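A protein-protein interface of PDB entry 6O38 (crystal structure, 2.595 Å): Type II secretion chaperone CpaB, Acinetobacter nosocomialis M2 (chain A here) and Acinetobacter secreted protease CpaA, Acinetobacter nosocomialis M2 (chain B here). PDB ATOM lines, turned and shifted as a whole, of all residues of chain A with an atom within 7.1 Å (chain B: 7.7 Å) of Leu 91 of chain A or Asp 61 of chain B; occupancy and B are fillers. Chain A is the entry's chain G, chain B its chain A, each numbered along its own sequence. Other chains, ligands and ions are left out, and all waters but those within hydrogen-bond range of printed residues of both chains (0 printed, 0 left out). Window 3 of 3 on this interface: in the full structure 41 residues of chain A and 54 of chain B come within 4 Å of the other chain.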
ATOM      1  N   GLU A  47      -5.947   0.317  35.752  1.00  0.00           N
ATOM      2  CA  GLU A  47      -5.323   1.630  35.710  1.00  0.00           C
ATOM      3  C   GLU A  47      -6.351   2.725  35.975  1.00  0.00           C
ATOM      4  O   GLU A  47      -7.551   2.564  35.740  1.00  0.00           O
ATOM      5  CB  GLU A  47      -4.661   1.878  34.355  1.00  0.00           C
ATOM      6  CG  GLU A  47      -3.238   1.378  34.233  1.00  0.00           C
ATOM      7  CD  GLU A  47      -2.389   2.279  33.355  1.00  0.00           C
ATOM      8  OE1 GLU A  47      -2.451   3.514  33.534  1.00  0.00           O
ATOM      9  OE2 GLU A  47      -1.662   1.756  32.484  1.00  0.00           O
ATOM     10  N   MET A  68       2.366   4.004  38.836  1.00  0.00           N
ATOM     11  CA  MET A  68       1.108   3.887  38.112  1.00  0.00           C
ATOM     12  C   MET A  68      -0.050   3.619  39.070  1.00  0.00           C
ATOM     13  O   MET A  68      -0.140   2.542  39.660  1.00  0.00           O
ATOM     14  CB  MET A  68       1.212   2.773  37.071  1.00  0.00           C
ATOM     15  CG  MET A  68       0.012   2.624  36.161  1.00  0.00           C
ATOM     16  SD  MET A  68       0.255   1.090  34.988  1.00  0.00           S
ATOM     17  CE  MET A  68       0.452  -0.278  36.357  1.00  0.00           C
ATOM     18  N   LYS A  87      -5.352 -12.422  35.625  1.00  0.00           N
ATOM     19  CA  LYS A  87      -4.795 -11.621  34.543  1.00  0.00           C
ATOM     20  C   LYS A  87      -4.241 -10.310  35.086  1.00  0.00           C
ATOM     21  O   LYS A  87      -4.839  -9.690  35.970  1.00  0.00           O
ATOM     22  CB  LYS A  87      -5.861 -11.337  33.478  1.00  0.00           C
ATOM     23  CG  LYS A  87      -5.335 -10.715  32.198  1.00  0.00           C
ATOM     24  CD  LYS A  87      -6.425 -10.687  31.139  1.00  0.00           C
ATOM     25  CE  LYS A  87      -5.844 -10.714  29.737  1.00  0.00           C
ATOM     26  NZ  LYS A  87      -6.898 -10.971  28.717  1.00  0.00           N
ATOM     27  N   PHE A  88      -3.098  -9.892  34.545  1.00  0.00           N
ATOM     28  CA  PHE A  88      -2.464  -8.629  34.896  1.00  0.00           C
ATOM     29  C   PHE A  88      -2.367  -7.748  33.657  1.00  0.00           C
ATOM     30  O   PHE A  88      -1.993  -8.221  32.579  1.00  0.00           O
ATOM     31  CB  PHE A  88      -1.062  -8.846  35.480  1.00  0.00           C
ATOM     32  CG  PHE A  88      -1.042  -9.689  36.721  1.00  0.00           C
ATOM     33  CD1 PHE A  88      -1.221  -9.115  37.970  1.00  0.00           C
ATOM     34  CD2 PHE A  88      -0.829 -11.057  36.643  1.00  0.00           C
ATOM     35  CE1 PHE A  88      -1.198  -9.889  39.115  1.00  0.00           C
ATOM     36  CE2 PHE A  88      -0.803 -11.835  37.784  1.00  0.00           C
ATOM     37  CZ  PHE A  88      -0.989 -11.251  39.021  1.00  0.00           C
ATOM     38  N   GLN A  89      -2.698  -6.467  33.814  1.00  0.00           N
ATOM     39  CA  GLN A  89      -2.617  -5.498  32.726  1.00  0.00           C
ATOM     40  C   GLN A  89      -1.824  -4.287  33.200  1.00  0.00           C
ATOM     41  O   GLN A  89      -2.291  -3.525  34.052  1.00  0.00           O
ATOM     42  CB  GLN A  89      -4.006  -5.086  32.239  1.00  0.00           C
ATOM     43  CG  GLN A  89      -4.649  -6.098  31.304  1.00  0.00           C
ATOM     44  CD  GLN A  89      -5.871  -5.549  30.597  1.00  0.00           C
ATOM     45  OE1 GLN A  89      -6.422  -4.521  30.992  1.00  0.00           O
ATOM     46  NE2 GLN A  89      -6.299  -6.230  29.542  1.00  0.00           N
ATOM     47  N   MET A  90      -0.626  -4.122  32.648  1.00  0.00           N
ATOM     48  CA  MET A  90       0.248  -2.995  32.952  1.00  0.00           C
ATOM     49  C   MET A  90       0.821  -2.440  31.651  1.00  0.00           C
ATOM     50  O   MET A  90       2.034  -2.285  31.513  1.00  0.00           O
ATOM     51  CB  MET A  90       1.360  -3.418  33.911  1.00  0.00           C
ATOM     52  CG  MET A  90       0.876  -3.629  35.337  1.00  0.00           C
ATOM     53  SD  MET A  90       2.117  -4.635  36.444  1.00  0.00           S
ATOM     54  CE  MET A  90       1.743  -6.410  35.739  1.00  0.00           C
ATOM     55  N   LEU A  91      -0.085  -2.167  30.705  1.00  0.00           N
ATOM     56  CA  LEU A  91       0.286  -1.909  29.313  1.00  0.00           C
ATOM     57  C   LEU A  91       1.422  -0.898  29.182  1.00  0.00           C
ATOM     58  O   LEU A  91       2.292  -1.049  28.315  1.00  0.00           O
ATOM     59  CB  LEU A  91      -0.938  -1.429  28.528  1.00  0.00           C
ATOM     60  CG  LEU A  91      -1.982  -2.469  28.103  1.00  0.00           C
ATOM     61  CD1 LEU A  91      -2.808  -2.972  29.282  1.00  0.00           C
ATOM     62  CD2 LEU A  91      -2.885  -1.900  27.017  1.00  0.00           C
ATOM     63  N   GLU A  92       1.432   0.142  30.022  1.00  0.00           N
ATOM     64  CA  GLU A  92       2.512   1.122  29.945  1.00  0.00           C
ATOM     65  C   GLU A  92       3.868   0.478  30.202  1.00  0.00           C
ATOM     66  O   GLU A  92       4.875   0.898  29.621  1.00  0.00           O
ATOM     67  CB  GLU A  92       2.276   2.261  30.936  1.00  0.00           C
ATOM     68  CG  GLU A  92       3.230   3.435  30.741  1.00  0.00           C
ATOM     69  CD  GLU A  92       3.462   4.227  32.012  1.00  0.00           C
ATOM     70  OE1 GLU A  92       2.816   3.918  33.035  1.00  0.00           O
ATOM     71  OE2 GLU A  92       4.297   5.156  31.987  1.00  0.00           O
ATOM     72  N   TYR A  93       3.912  -0.539  31.057  1.00  0.00           N
ATOM     73  CA  TYR A  93       5.130  -1.295  31.312  1.00  0.00           C
ATOM     74  C   TYR A  93       5.282  -2.491  30.380  1.00  0.00           C
ATOM     75  O   TYR A  93       6.228  -3.268  30.543  1.00  0.00           O
ATOM     76  CB  TYR A  93       5.160  -1.770  32.768  1.00  0.00           C
ATOM     77  CG  TYR A  93       5.170  -0.648  33.781  1.00  0.00           C
ATOM     78  CD1 TYR A  93       5.709   0.594  33.467  1.00  0.00           C
ATOM     79  CD2 TYR A  93       4.639  -0.828  35.051  1.00  0.00           C
ATOM     80  CE1 TYR A  93       5.719   1.623  34.391  1.00  0.00           C
ATOM     81  CE2 TYR A  93       4.645   0.194  35.982  1.00  0.00           C
ATOM     82  CZ  TYR A  93       5.187   1.417  35.647  1.00  0.00           C
ATOM     83  OH  TYR A  93       5.196   2.438  36.570  1.00  0.00           O
ATOM     84  N   GLY A  94       4.378  -2.656  29.417  1.00  0.00           N
ATOM     85  CA  GLY A  94       4.481  -3.739  28.463  1.00  0.00           C
ATOM     86  C   GLY A  94       4.103  -5.104  28.987  1.00  0.00           C
ATOM     87  O   GLY A  94       4.558  -6.111  28.436  1.00  0.00           O
ATOM     88  N   ILE A  95       3.283  -5.177  30.031  1.00  0.00           N
ATOM     89  CA  ILE A  95       2.884  -6.443  30.636  1.00  0.00           C
ATOM     90  C   ILE A  95       1.395  -6.644  30.398  1.00  0.00           C
ATOM     91  O   ILE A  95       0.568  -5.854  30.870  1.00  0.00           O
ATOM     92  CB  ILE A  95       3.210  -6.487  32.136  1.00  0.00           C
ATOM     93  CG1 ILE A  95       4.685  -6.162  32.365  1.00  0.00           C
ATOM     94  CG2 ILE A  95       2.881  -7.857  32.701  1.00  0.00           C
ATOM     95  CD1 ILE A  95       5.635  -7.148  31.723  1.00  0.00           C
ATOM     96  N   ASN A  96       1.057  -7.704  29.664  1.00  0.00           N
ATOM     97  CA  ASN A  96      -0.337  -8.073  29.408  1.00  0.00           C
ATOM     98  C   ASN A  96      -0.369  -9.595  29.259  1.00  0.00           C
ATOM     99  O   ASN A  96      -0.129 -10.129  28.175  1.00  0.00           O
ATOM    100  CB  ASN A  96      -0.878  -7.370  28.171  1.00  0.00           C
ATOM    101  CG  ASN A  96      -2.326  -7.710  27.894  1.00  0.00           C
ATOM    102  OD1 ASN A  96      -3.107  -7.952  28.814  1.00  0.00           O
ATOM    103  ND2 ASN A  96      -2.691  -7.736  26.620  1.00  0.00           N
ATOM    104  N   GLY B  14     -10.886   3.299  25.496  1.00  0.00           N
ATOM    105  CA  GLY B  14      -9.993   2.773  24.487  1.00  0.00           C
ATOM    106  C   GLY B  14     -10.456   1.506  23.813  1.00  0.00           C
ATOM    107  O   GLY B  14      -9.799   1.032  22.883  1.00  0.00           O
ATOM    108  N   LYS B  34      -5.235   6.226  27.365  1.00  0.00           N
ATOM    109  CA  LYS B  34      -3.928   5.592  27.506  1.00  0.00           C
ATOM    110  C   LYS B  34      -3.926   4.168  26.958  1.00  0.00           C
ATOM    111  O   LYS B  34      -3.045   3.801  26.171  1.00  0.00           O
ATOM    112  CB  LYS B  34      -3.495   5.600  28.974  1.00  0.00           C
ATOM    113  CG  LYS B  34      -2.005   5.374  29.171  1.00  0.00           C
ATOM    114  CD  LYS B  34      -1.616   5.472  30.637  1.00  0.00           C
ATOM    115  CE  LYS B  34      -0.111   5.630  30.794  1.00  0.00           C
ATOM    116  NZ  LYS B  34       0.376   6.890  30.163  1.00  0.00           N
ATOM    117  N   ASN B  35      -4.897   3.355  27.358  1.00  0.00           N
ATOM    118  CA  ASN B  35      -4.942   1.944  26.993  1.00  0.00           C
ATOM    119  C   ASN B  35      -6.007   1.713  25.930  1.00  0.00           C
ATOM    120  O   ASN B  35      -7.146   2.168  26.076  1.00  0.00           O
ATOM    121  CB  ASN B  35      -5.215   1.075  28.223  1.00  0.00           C
ATOM    122  CG  ASN B  35      -4.144   1.221  29.287  1.00  0.00           C
ATOM    123  OD1 ASN B  35      -2.976   1.460  28.980  1.00  0.00           O
ATOM    124  ND2 ASN B  35      -4.539   1.079  30.547  1.00  0.00           N
ATOM    125  N   LEU B  36      -5.630   1.006  24.867  1.00  0.00           N
ATOM    126  CA  LEU B  36      -6.516   0.706  23.754  1.00  0.00           C
ATOM    127  C   LEU B  36      -6.576  -0.800  23.533  1.00  0.00           C
ATOM    128  O   LEU B  36      -5.672  -1.544  23.923  1.00  0.00           O
ATOM    129  CB  LEU B  36      -6.055   1.401  22.463  1.00  0.00           C
ATOM    130  CG  LEU B  36      -6.226   2.917  22.319  1.00  0.00           C
ATOM    131  CD1 LEU B  36      -5.236   3.687  23.181  1.00  0.00           C
ATOM    132  CD2 LEU B  36      -6.092   3.326  20.860  1.00  0.00           C
ATOM    133  N   SER B  37      -7.656  -1.243  22.894  1.00  0.00           N
ATOM    134  CA  SER B  37      -7.837  -2.655  22.594  1.00  0.00           C
ATOM    135  C   SER B  37      -8.748  -2.799  21.385  1.00  0.00           C
ATOM    136  O   SER B  37      -9.607  -1.951  21.131  1.00  0.00           O
ATOM    137  CB  SER B  37      -8.420  -3.419  23.789  1.00  0.00           C
ATOM    138  OG  SER B  37      -9.725  -2.961  24.098  1.00  0.00           O
ATOM    139  N   LEU B  38      -8.547  -3.890  20.638  1.00  0.00           N
ATOM    140  CA  LEU B  38      -9.341  -4.243  19.473  1.00  0.00           C
ATOM    141  C   LEU B  38     -10.482  -5.177  19.870  1.00  0.00           C
ATOM    142  O   LEU B  38     -10.352  -5.956  20.821  1.00  0.00           O
ATOM    143  CB  LEU B  38      -8.467  -4.915  18.417  1.00  0.00           C
ATOM    144  CG  LEU B  38      -7.320  -4.065  17.864  1.00  0.00           C
ATOM    145  CD1 LEU B  38      -6.486  -4.862  16.875  1.00  0.00           C
ATOM    146  CD2 LEU B  38      -7.853  -2.794  17.219  1.00  0.00           C
ATOM    147  N   THR B  40     -13.028  -8.294  20.068  1.00  0.00           N
ATOM    148  CA  THR B  40     -12.956  -9.726  19.797  1.00  0.00           C
ATOM    149  C   THR B  40     -13.997 -10.144  18.766  1.00  0.00           C
ATOM    150  O   THR B  40     -13.687 -10.879  17.821  1.00  0.00           O
ATOM    151  CB  THR B  40     -13.135 -10.519  21.095  1.00  0.00           C
ATOM    152  OG1 THR B  40     -14.174  -9.924  21.882  1.00  0.00           O
ATOM    153  CG2 THR B  40     -11.839 -10.535  21.893  1.00  0.00           C
ATOM    154  N   ILE B  50      -5.519   2.832  13.501  1.00  0.00           N
ATOM    155  CA  ILE B  50      -5.288   3.651  14.686  1.00  0.00           C
ATOM    156  C   ILE B  50      -4.275   4.731  14.330  1.00  0.00           C
ATOM    157  O   ILE B  50      -3.152   4.426  13.910  1.00  0.00           O
ATOM    158  CB  ILE B  50      -4.798   2.808  15.873  1.00  0.00           C
ATOM    159  CG1 ILE B  50      -5.792   1.689  16.184  1.00  0.00           C
ATOM    160  CG2 ILE B  50      -4.585   3.686  17.096  1.00  0.00           C
ATOM    161  CD1 ILE B  50      -5.347   0.774  17.306  1.00  0.00           C
ATOM    162  N   SER B  58       0.223   6.134  23.750  1.00  0.00           N
ATOM    163  CA  SER B  58      -0.847   5.184  24.001  1.00  0.00           C
ATOM    164  C   SER B  58      -0.311   3.767  23.848  1.00  0.00           C
ATOM    165  O   SER B  58       0.742   3.539  23.245  1.00  0.00           O
ATOM    166  CB  SER B  58      -2.030   5.410  23.052  1.00  0.00           C
ATOM    167  OG  SER B  58      -2.636   6.670  23.287  1.00  0.00           O
ATOM    168  N   TYR B  59      -1.047   2.810  24.406  1.00  0.00           N
ATOM    169  CA  TYR B  59      -0.616   1.419  24.443  1.00  0.00           C
ATOM    170  C   TYR B  59      -1.775   0.520  24.044  1.00  0.00           C
ATOM    171  O   TYR B  59      -2.886   0.665  24.563  1.00  0.00           O
ATOM    172  CB  TYR B  59      -0.088   1.055  25.834  1.00  0.00           C
ATOM    173  CG  TYR B  59       1.057   1.938  26.273  1.00  0.00           C
ATOM    174  CD1 TYR B  59       2.367   1.631  25.929  1.00  0.00           C
ATOM    175  CD2 TYR B  59       0.828   3.088  27.016  1.00  0.00           C
ATOM    176  CE1 TYR B  59       3.417   2.439  26.322  1.00  0.00           C
ATOM    177  CE2 TYR B  59       1.872   3.903  27.413  1.00  0.00           C
ATOM    178  CZ  TYR B  59       3.164   3.573  27.063  1.00  0.00           C
ATOM    179  OH  TYR B  59       4.206   4.382  27.456  1.00  0.00           O
ATOM    180  N   LEU B  60      -1.511  -0.404  23.125  1.00  0.00           N
ATOM    181  CA  LEU B  60      -2.539  -1.241  22.522  1.00  0.00           C
ATOM    182  C   LEU B  60      -2.410  -2.676  23.016  1.00  0.00           C
ATOM    183  O   LEU B  60      -1.322  -3.260  22.965  1.00  0.00           O
ATOM    184  CB  LEU B  60      -2.441  -1.204  20.995  1.00  0.00           C
ATOM    185  CG  LEU B  60      -3.360  -2.161  20.231  1.00  0.00           C
ATOM    186  CD1 LEU B  60      -4.821  -1.845  20.511  1.00  0.00           C
ATOM    187  CD2 LEU B  60      -3.072  -2.109  18.739  1.00  0.00           C
ATOM    188  N   ASP B  61      -3.521  -3.233  23.490  1.00  0.00           N
ATOM    189  CA  ASP B  61      -3.582  -4.650  23.826  1.00  0.00           C
ATOM    190  C   ASP B  61      -3.480  -5.475  22.548  1.00  0.00           C
ATOM    191  O   ASP B  61      -4.292  -5.313  21.630  1.00  0.00           O
ATOM    192  CB  ASP B  61      -4.882  -4.953  24.569  1.00  0.00           C
ATOM    193  CG  ASP B  61      -5.019  -6.418  24.947  1.00  0.00           C
ATOM    194  OD1 ASP B  61      -4.025  -7.167  24.853  1.00  0.00           O
ATOM    195  OD2 ASP B  61      -6.134  -6.822  25.342  1.00  0.00           O
ATOM    196  N   THR B  62      -2.483  -6.359  22.486  1.00  0.00           N
ATOM    197  CA  THR B  62      -2.219  -7.161  21.298  1.00  0.00           C
ATOM    198  C   THR B  62      -2.567  -8.631  21.501  1.00  0.00           C
ATOM    199  O   THR B  62      -2.102  -9.484  20.738  1.00  0.00           O
ATOM    200  CB  THR B  62      -0.754  -7.022  20.882  1.00  0.00           C
ATOM    201  OG1 THR B  62       0.084  -7.609  21.885  1.00  0.00           O
ATOM    202  CG2 THR B  62      -0.391  -5.560  20.728  1.00  0.00           C
ATOM    203  N   SER B  63      -3.381  -8.942  22.512  1.00  0.00           N
ATOM    204  CA  SER B  63      -3.647 -10.338  22.845  1.00  0.00           C
ATOM    205  C   SER B  63      -4.482 -11.036  21.778  1.00  0.00           C
ATOM    206  O   SER B  63      -4.410 -12.262  21.645  1.00  0.00           O
ATOM    207  CB  SER B  63      -4.342 -10.429  24.203  1.00  0.00           C
ATOM    208  OG  SER B  63      -5.532  -9.660  24.220  1.00  0.00           O
ATOM    209  N   ASN B  64      -5.277 -10.285  21.013  1.00  0.00           N
ATOM    210  CA  ASN B  64      -6.117 -10.855  19.967  1.00  0.00           C
ATOM    211  C   ASN B  64      -5.620 -10.484  18.572  1.00  0.00           C
ATOM    212  O   ASN B  64      -6.405 -10.418  17.622  1.00  0.00           O
ATOM    213  CB  ASN B  64      -7.572 -10.428  20.156  1.00  0.00           C
ATOM    214  CG  ASN B  64      -7.759  -8.927  20.063  1.00  0.00           C
ATOM    215  OD1 ASN B  64      -6.811  -8.156  20.216  1.00  0.00           O
ATOM    216  ND2 ASN B  64      -8.993  -8.502  19.816  1.00  0.00           N
ATOM    217  N   THR B  65      -4.322 -10.239  18.438  1.00  0.00           N
ATOM    218  CA  THR B  65      -3.681  -9.960  17.162  1.00  0.00           C
ATOM    219  C   THR B  65      -2.656 -11.052  16.864  1.00  0.00           C
ATOM    220  O   THR B  65      -2.500 -12.012  17.623  1.00  0.00           O
ATOM    221  CB  THR B  65      -3.014  -8.581  17.169  1.00  0.00           C
ATOM    222  OG1 THR B  65      -1.877  -8.603  18.041  1.00  0.00           O
ATOM    223  CG2 THR B  65      -3.990  -7.520  17.651  1.00  0.00           C
ATOM    224  N   LEU B  69       4.441  -9.409  20.236  1.00  0.00           N
ATOM    225  CA  LEU B  69       4.703  -8.522  21.358  1.00  0.00           C
ATOM    226  C   LEU B  69       3.465  -8.404  22.238  1.00  0.00           C
ATOM    227  O   LEU B  69       2.330  -8.538  21.772  1.00  0.00           O
ATOM    228  CB  LEU B  69       5.131  -7.139  20.864  1.00  0.00           C
ATOM    229  CG  LEU B  69       6.300  -7.096  19.875  1.00  0.00           C
ATOM    230  CD1 LEU B  69       6.665  -5.659  19.531  1.00  0.00           C
ATOM    231  CD2 LEU B  69       7.506  -7.842  20.423  1.00  0.00           C
ATOM    232  N   GLU B  70       3.692  -8.156  23.529  1.00  0.00           N
ATOM    233  CA  GLU B  70       2.575  -8.070  24.464  1.00  0.00           C
ATOM    234  C   GLU B  70       1.819  -6.754  24.327  1.00  0.00           C
ATOM    235  O   GLU B  70       0.585  -6.738  24.392  1.00  0.00           O
ATOM    236  CB  GLU B  70       3.069  -8.257  25.898  1.00  0.00           C
ATOM    237  CG  GLU B  70       2.790  -9.642  26.464  1.00  0.00           C
ATOM    238  CD  GLU B  70       3.386  -9.851  27.842  1.00  0.00           C
ATOM    239  OE1 GLU B  70       3.769  -8.854  28.489  1.00  0.00           O
ATOM    240  OE2 GLU B  70       3.476 -11.018  28.276  1.00  0.00           O
ATOM    241  N   VAL B  71       2.531  -5.645  24.144  1.00  0.00           N
ATOM    242  CA  VAL B  71       1.921  -4.322  24.061  1.00  0.00           C
ATOM    243  C   VAL B  71       2.568  -3.557  22.914  1.00  0.00           C
ATOM    244  O   VAL B  71       3.776  -3.673  22.679  1.00  0.00           O
ATOM    245  CB  VAL B  71       2.067  -3.544  25.389  1.00  0.00           C
ATOM    246  CG1 VAL B  71       1.449  -2.160  25.276  1.00  0.00           C
ATOM    247  CG2 VAL B  71       1.432  -4.312  26.541  1.00  0.00           C
ATOM    248  N   LEU B  72       1.760  -2.783  22.190  1.00  0.00           N
ATOM    249  CA  LEU B  72       2.251  -1.878  21.160  1.00  0.00           C
ATOM    250  C   LEU B  72       2.285  -0.457  21.705  1.00  0.00           C
ATOM    251  O   LEU B  72       1.286   0.030  22.243  1.00  0.00           O
ATOM    252  CB  LEU B  72       1.376  -1.927  19.906  1.00  0.00           C
ATOM    253  CG  LEU B  72       1.515  -3.119  18.959  1.00  0.00           C
ATOM    254  CD1 LEU B  72       1.359  -2.656  17.519  1.00  0.00           C
ATOM    255  CD2 LEU B  72       2.837  -3.844  19.163  1.00  0.00           C
ATOM    256  N   LYS B  73       3.430   0.203  21.557  1.00  0.00           N
ATOM    257  CA  LYS B  73       3.582   1.593  21.966  1.00  0.00           C
ATOM    258  C   LYS B  73       3.151   2.494  20.815  1.00  0.00           C
ATOM    259  O   LYS B  73       3.749   2.457  19.734  1.00  0.00           O
ATOM    260  CB  LYS B  73       5.026   1.883  22.373  1.00  0.00           C
ATOM    261  CG  LYS B  73       5.220   3.192  23.124  1.00  0.00           C
ATOM    262  CD  LYS B  73       6.674   3.370  23.539  1.00  0.00           C
ATOM    263  CE  LYS B  73       6.840   4.497  24.549  1.00  0.00           C
ATOM    264  NZ  LYS B  73       6.473   5.825  23.987  1.00  0.00           N
ATOM    265  N   ILE B  74       2.115   3.295  21.045  1.00  0.00           N
ATOM    266  CA  ILE B  74       1.579   4.203  20.037  1.00  0.00           C
ATOM    267  C   ILE B  74       2.079   5.606  20.345  1.00  0.00           C
ATOM    268  O   ILE B  74       1.818   6.143  21.427  1.00  0.00           O
ATOM    269  CB  ILE B  74       0.043   4.158  20.001  1.00  0.00           C
ATOM    270  CG1 ILE B  74      -0.445   2.764  19.604  1.00  0.00           C
ATOM    271  CG2 ILE B  74      -0.496   5.204  19.043  1.00  0.00           C
ATOM    272  CD1 ILE B  74      -1.952   2.640  19.539  1.00  0.00           C
ATOM    273  N   PHE B  82      -5.014  -2.799  11.009  1.00  0.00           N
ATOM    274  CA  PHE B  82      -5.304  -4.200  11.273  1.00  0.00           C
ATOM    275  C   PHE B  82      -6.461  -4.661  10.401  1.00  0.00           C
ATOM    276  O   PHE B  82      -7.402  -3.903  10.149  1.00  0.00           O
ATOM    277  CB  PHE B  82      -5.644  -4.435  12.751  1.00  0.00           C
ATOM    278  CG  PHE B  82      -4.514  -4.135  13.692  1.00  0.00           C
ATOM    279  CD1 PHE B  82      -3.591  -5.113  14.022  1.00  0.00           C
ATOM    280  CD2 PHE B  82      -4.378  -2.875  14.252  1.00  0.00           C
ATOM    281  CE1 PHE B  82      -2.551  -4.840  14.890  1.00  0.00           C
ATOM    282  CE2 PHE B  82      -3.339  -2.596  15.120  1.00  0.00           C
ATOM    283  CZ  PHE B  82      -2.426  -3.580  15.439  1.00  0.00           C
ATOM    284  N   TRP B  91      -6.713 -10.313  14.663  1.00  0.00           N
ATOM    285  CA  TRP B  91      -6.496  -9.134  13.836  1.00  0.00           C
ATOM    286  C   TRP B  91      -5.092  -9.194  13.246  1.00  0.00           C
ATOM    287  O   TRP B  91      -4.102  -9.154  13.985  1.00  0.00           O
ATOM    288  CB  TRP B  91      -6.680  -7.853  14.650  1.00  0.00           C
ATOM    289  CG  TRP B  91      -8.105  -7.545  15.005  1.00  0.00           C
ATOM    290  CD1 TRP B  91      -8.763  -7.905  16.144  1.00  0.00           C
ATOM    291  CD2 TRP B  91      -9.044  -6.801  14.218  1.00  0.00           C
ATOM    292  NE1 TRP B  91     -10.054  -7.437  16.114  1.00  0.00           N
ATOM    293  CE2 TRP B  91     -10.252  -6.755  14.942  1.00  0.00           C
ATOM    294  CE3 TRP B  91      -8.980  -6.171  12.971  1.00  0.00           C
ATOM    295  CZ2 TRP B  91     -11.387  -6.106  14.460  1.00  0.00           C
ATOM    296  CZ3 TRP B  91     -10.109  -5.527  12.495  1.00  0.00           C
ATOM    297  CH2 TRP B  91     -11.296  -5.502  13.237  1.00  0.00           C
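The side-chain carboxylate (OE1) of Glu 70 of chain B is in hydrogen-bond range of the backbone NH (N) of Asn 96 of chain A (3.2 Å). The side-chain amide nitrogen (ND2) of Asn 96 of chain A sits close to the side-chain carboxylate (OD1) of Asp 61 of chain B (2.3 Å). O of Gly 94 of chain A lies close to OE1 of Glu 70 of chain B, 2.9 Å away.
The backbone carbonyl oxygen (O) of Ile 95 of chain A lies within hydrogen-bond range of the backbone NH (N) of Met 90 of chain A, 2.8 Å away. The backbone carbonyl oxygen (O) of Leu 36 of chain B lies within hydrogen-bond range of the backbone NH (N) of Asp 61 of chain B. O of Glu 70 of chain B is in hydrogen-bond range of OG1 of Thr 62 of chain B (2.7 Å). O of Tyr 59 of chain B is in hydrogen-bond range of N of Leu 36 of chain B. OD1 of Asp 61 of chain B lies within hydrogen-bond range of OG of Ser 63 of chain B (3.0 Å). The backbone carbonyl oxygen of Lys 34 of chain B sits at hydrogen-bond distance from the backbone NH of Tyr 59 of chain B, at 2.8 Å.
Among the printed residues, pairs that only touch across the chains: Leu 91 of chain A with Val 71 of chain B (3.3 Å), Ile 95 of chain A with Glu 70 of chain B (3.3 Å), Glu 47 of chain A with Asn 35 of chain B (3.5 Å), Leu 91 of chain A with Tyr 59 of chain B (3.5 Å), Glu 92 of chain A with Tyr 59 of chain B (3.6 Å), Leu 91 of chain A with Asn 35 of chain B (3.6 Å), Glu 47 of chain A with Lys 34 of chain B (3.6 Å), Gly 94 of chain A with Val 71 of chain B (3.6 Å), Leu 91 of chain A with Asp 61 of chain B (3.8 Å), Asn 96 of chain A with Ser 63 of chain B (3.98 Å) and Glu 92 of chain A with Lys 34 of chain B (3.998 Å).
Of the printed residues of chain B, Leu 91 of chain A touches Asn 35, Tyr 59, Asp 61 and Val 71. Printed residues of chain B within 4 Å of Glu 92 of chain A: Lys 34 and Tyr 59. Printed residues of chain B within 4 Å of Asn 96 of chain A: Asp 61, Ser 63 and Glu 70. Gly 14 of chain B touches none of the printed residues of chain A. Of the printed residues of chain A, Lys 34 of chain B touches Glu 47 (3.6 Å) and Glu 92 (3.998 Å). Asp 61 of chain B touches just these residues of chain A: Leu 91 and Asn 96. Asn 64 of chain B touches none of the printed residues of chain A. The nearest residue of chain B that does not touch Leu 91 of chain A is Leu 60 of chain B (4.1 Å). The nearest residue of chain A that does not touch Asp 61 of chain B is Gln 89 of chain A (4.2 Å). The nearest printed residue of chain A that does not touch Val 71 of chain B is Ile 95 of chain A (4.04 Å).
Printed residues of chain B that touch a printed residue of chain A: Lys 34, Asn 35, Tyr 59, Asp 61, Ser 63, Glu 70 and Val 71. Of the 12 printed residues of chain A, 6 touch a printed residue of chain B. Printed residues of chain A that touch a printed residue of chain B: Glu 47, Leu 91, Glu 92, Gly 94, Ile 95 and Asn 96. Hydrophobic or aromatic side chains of chain A within 4 Å of the printed part of chain B: Leu 91. Among the printed residues, 14 pairs touch across the chains.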
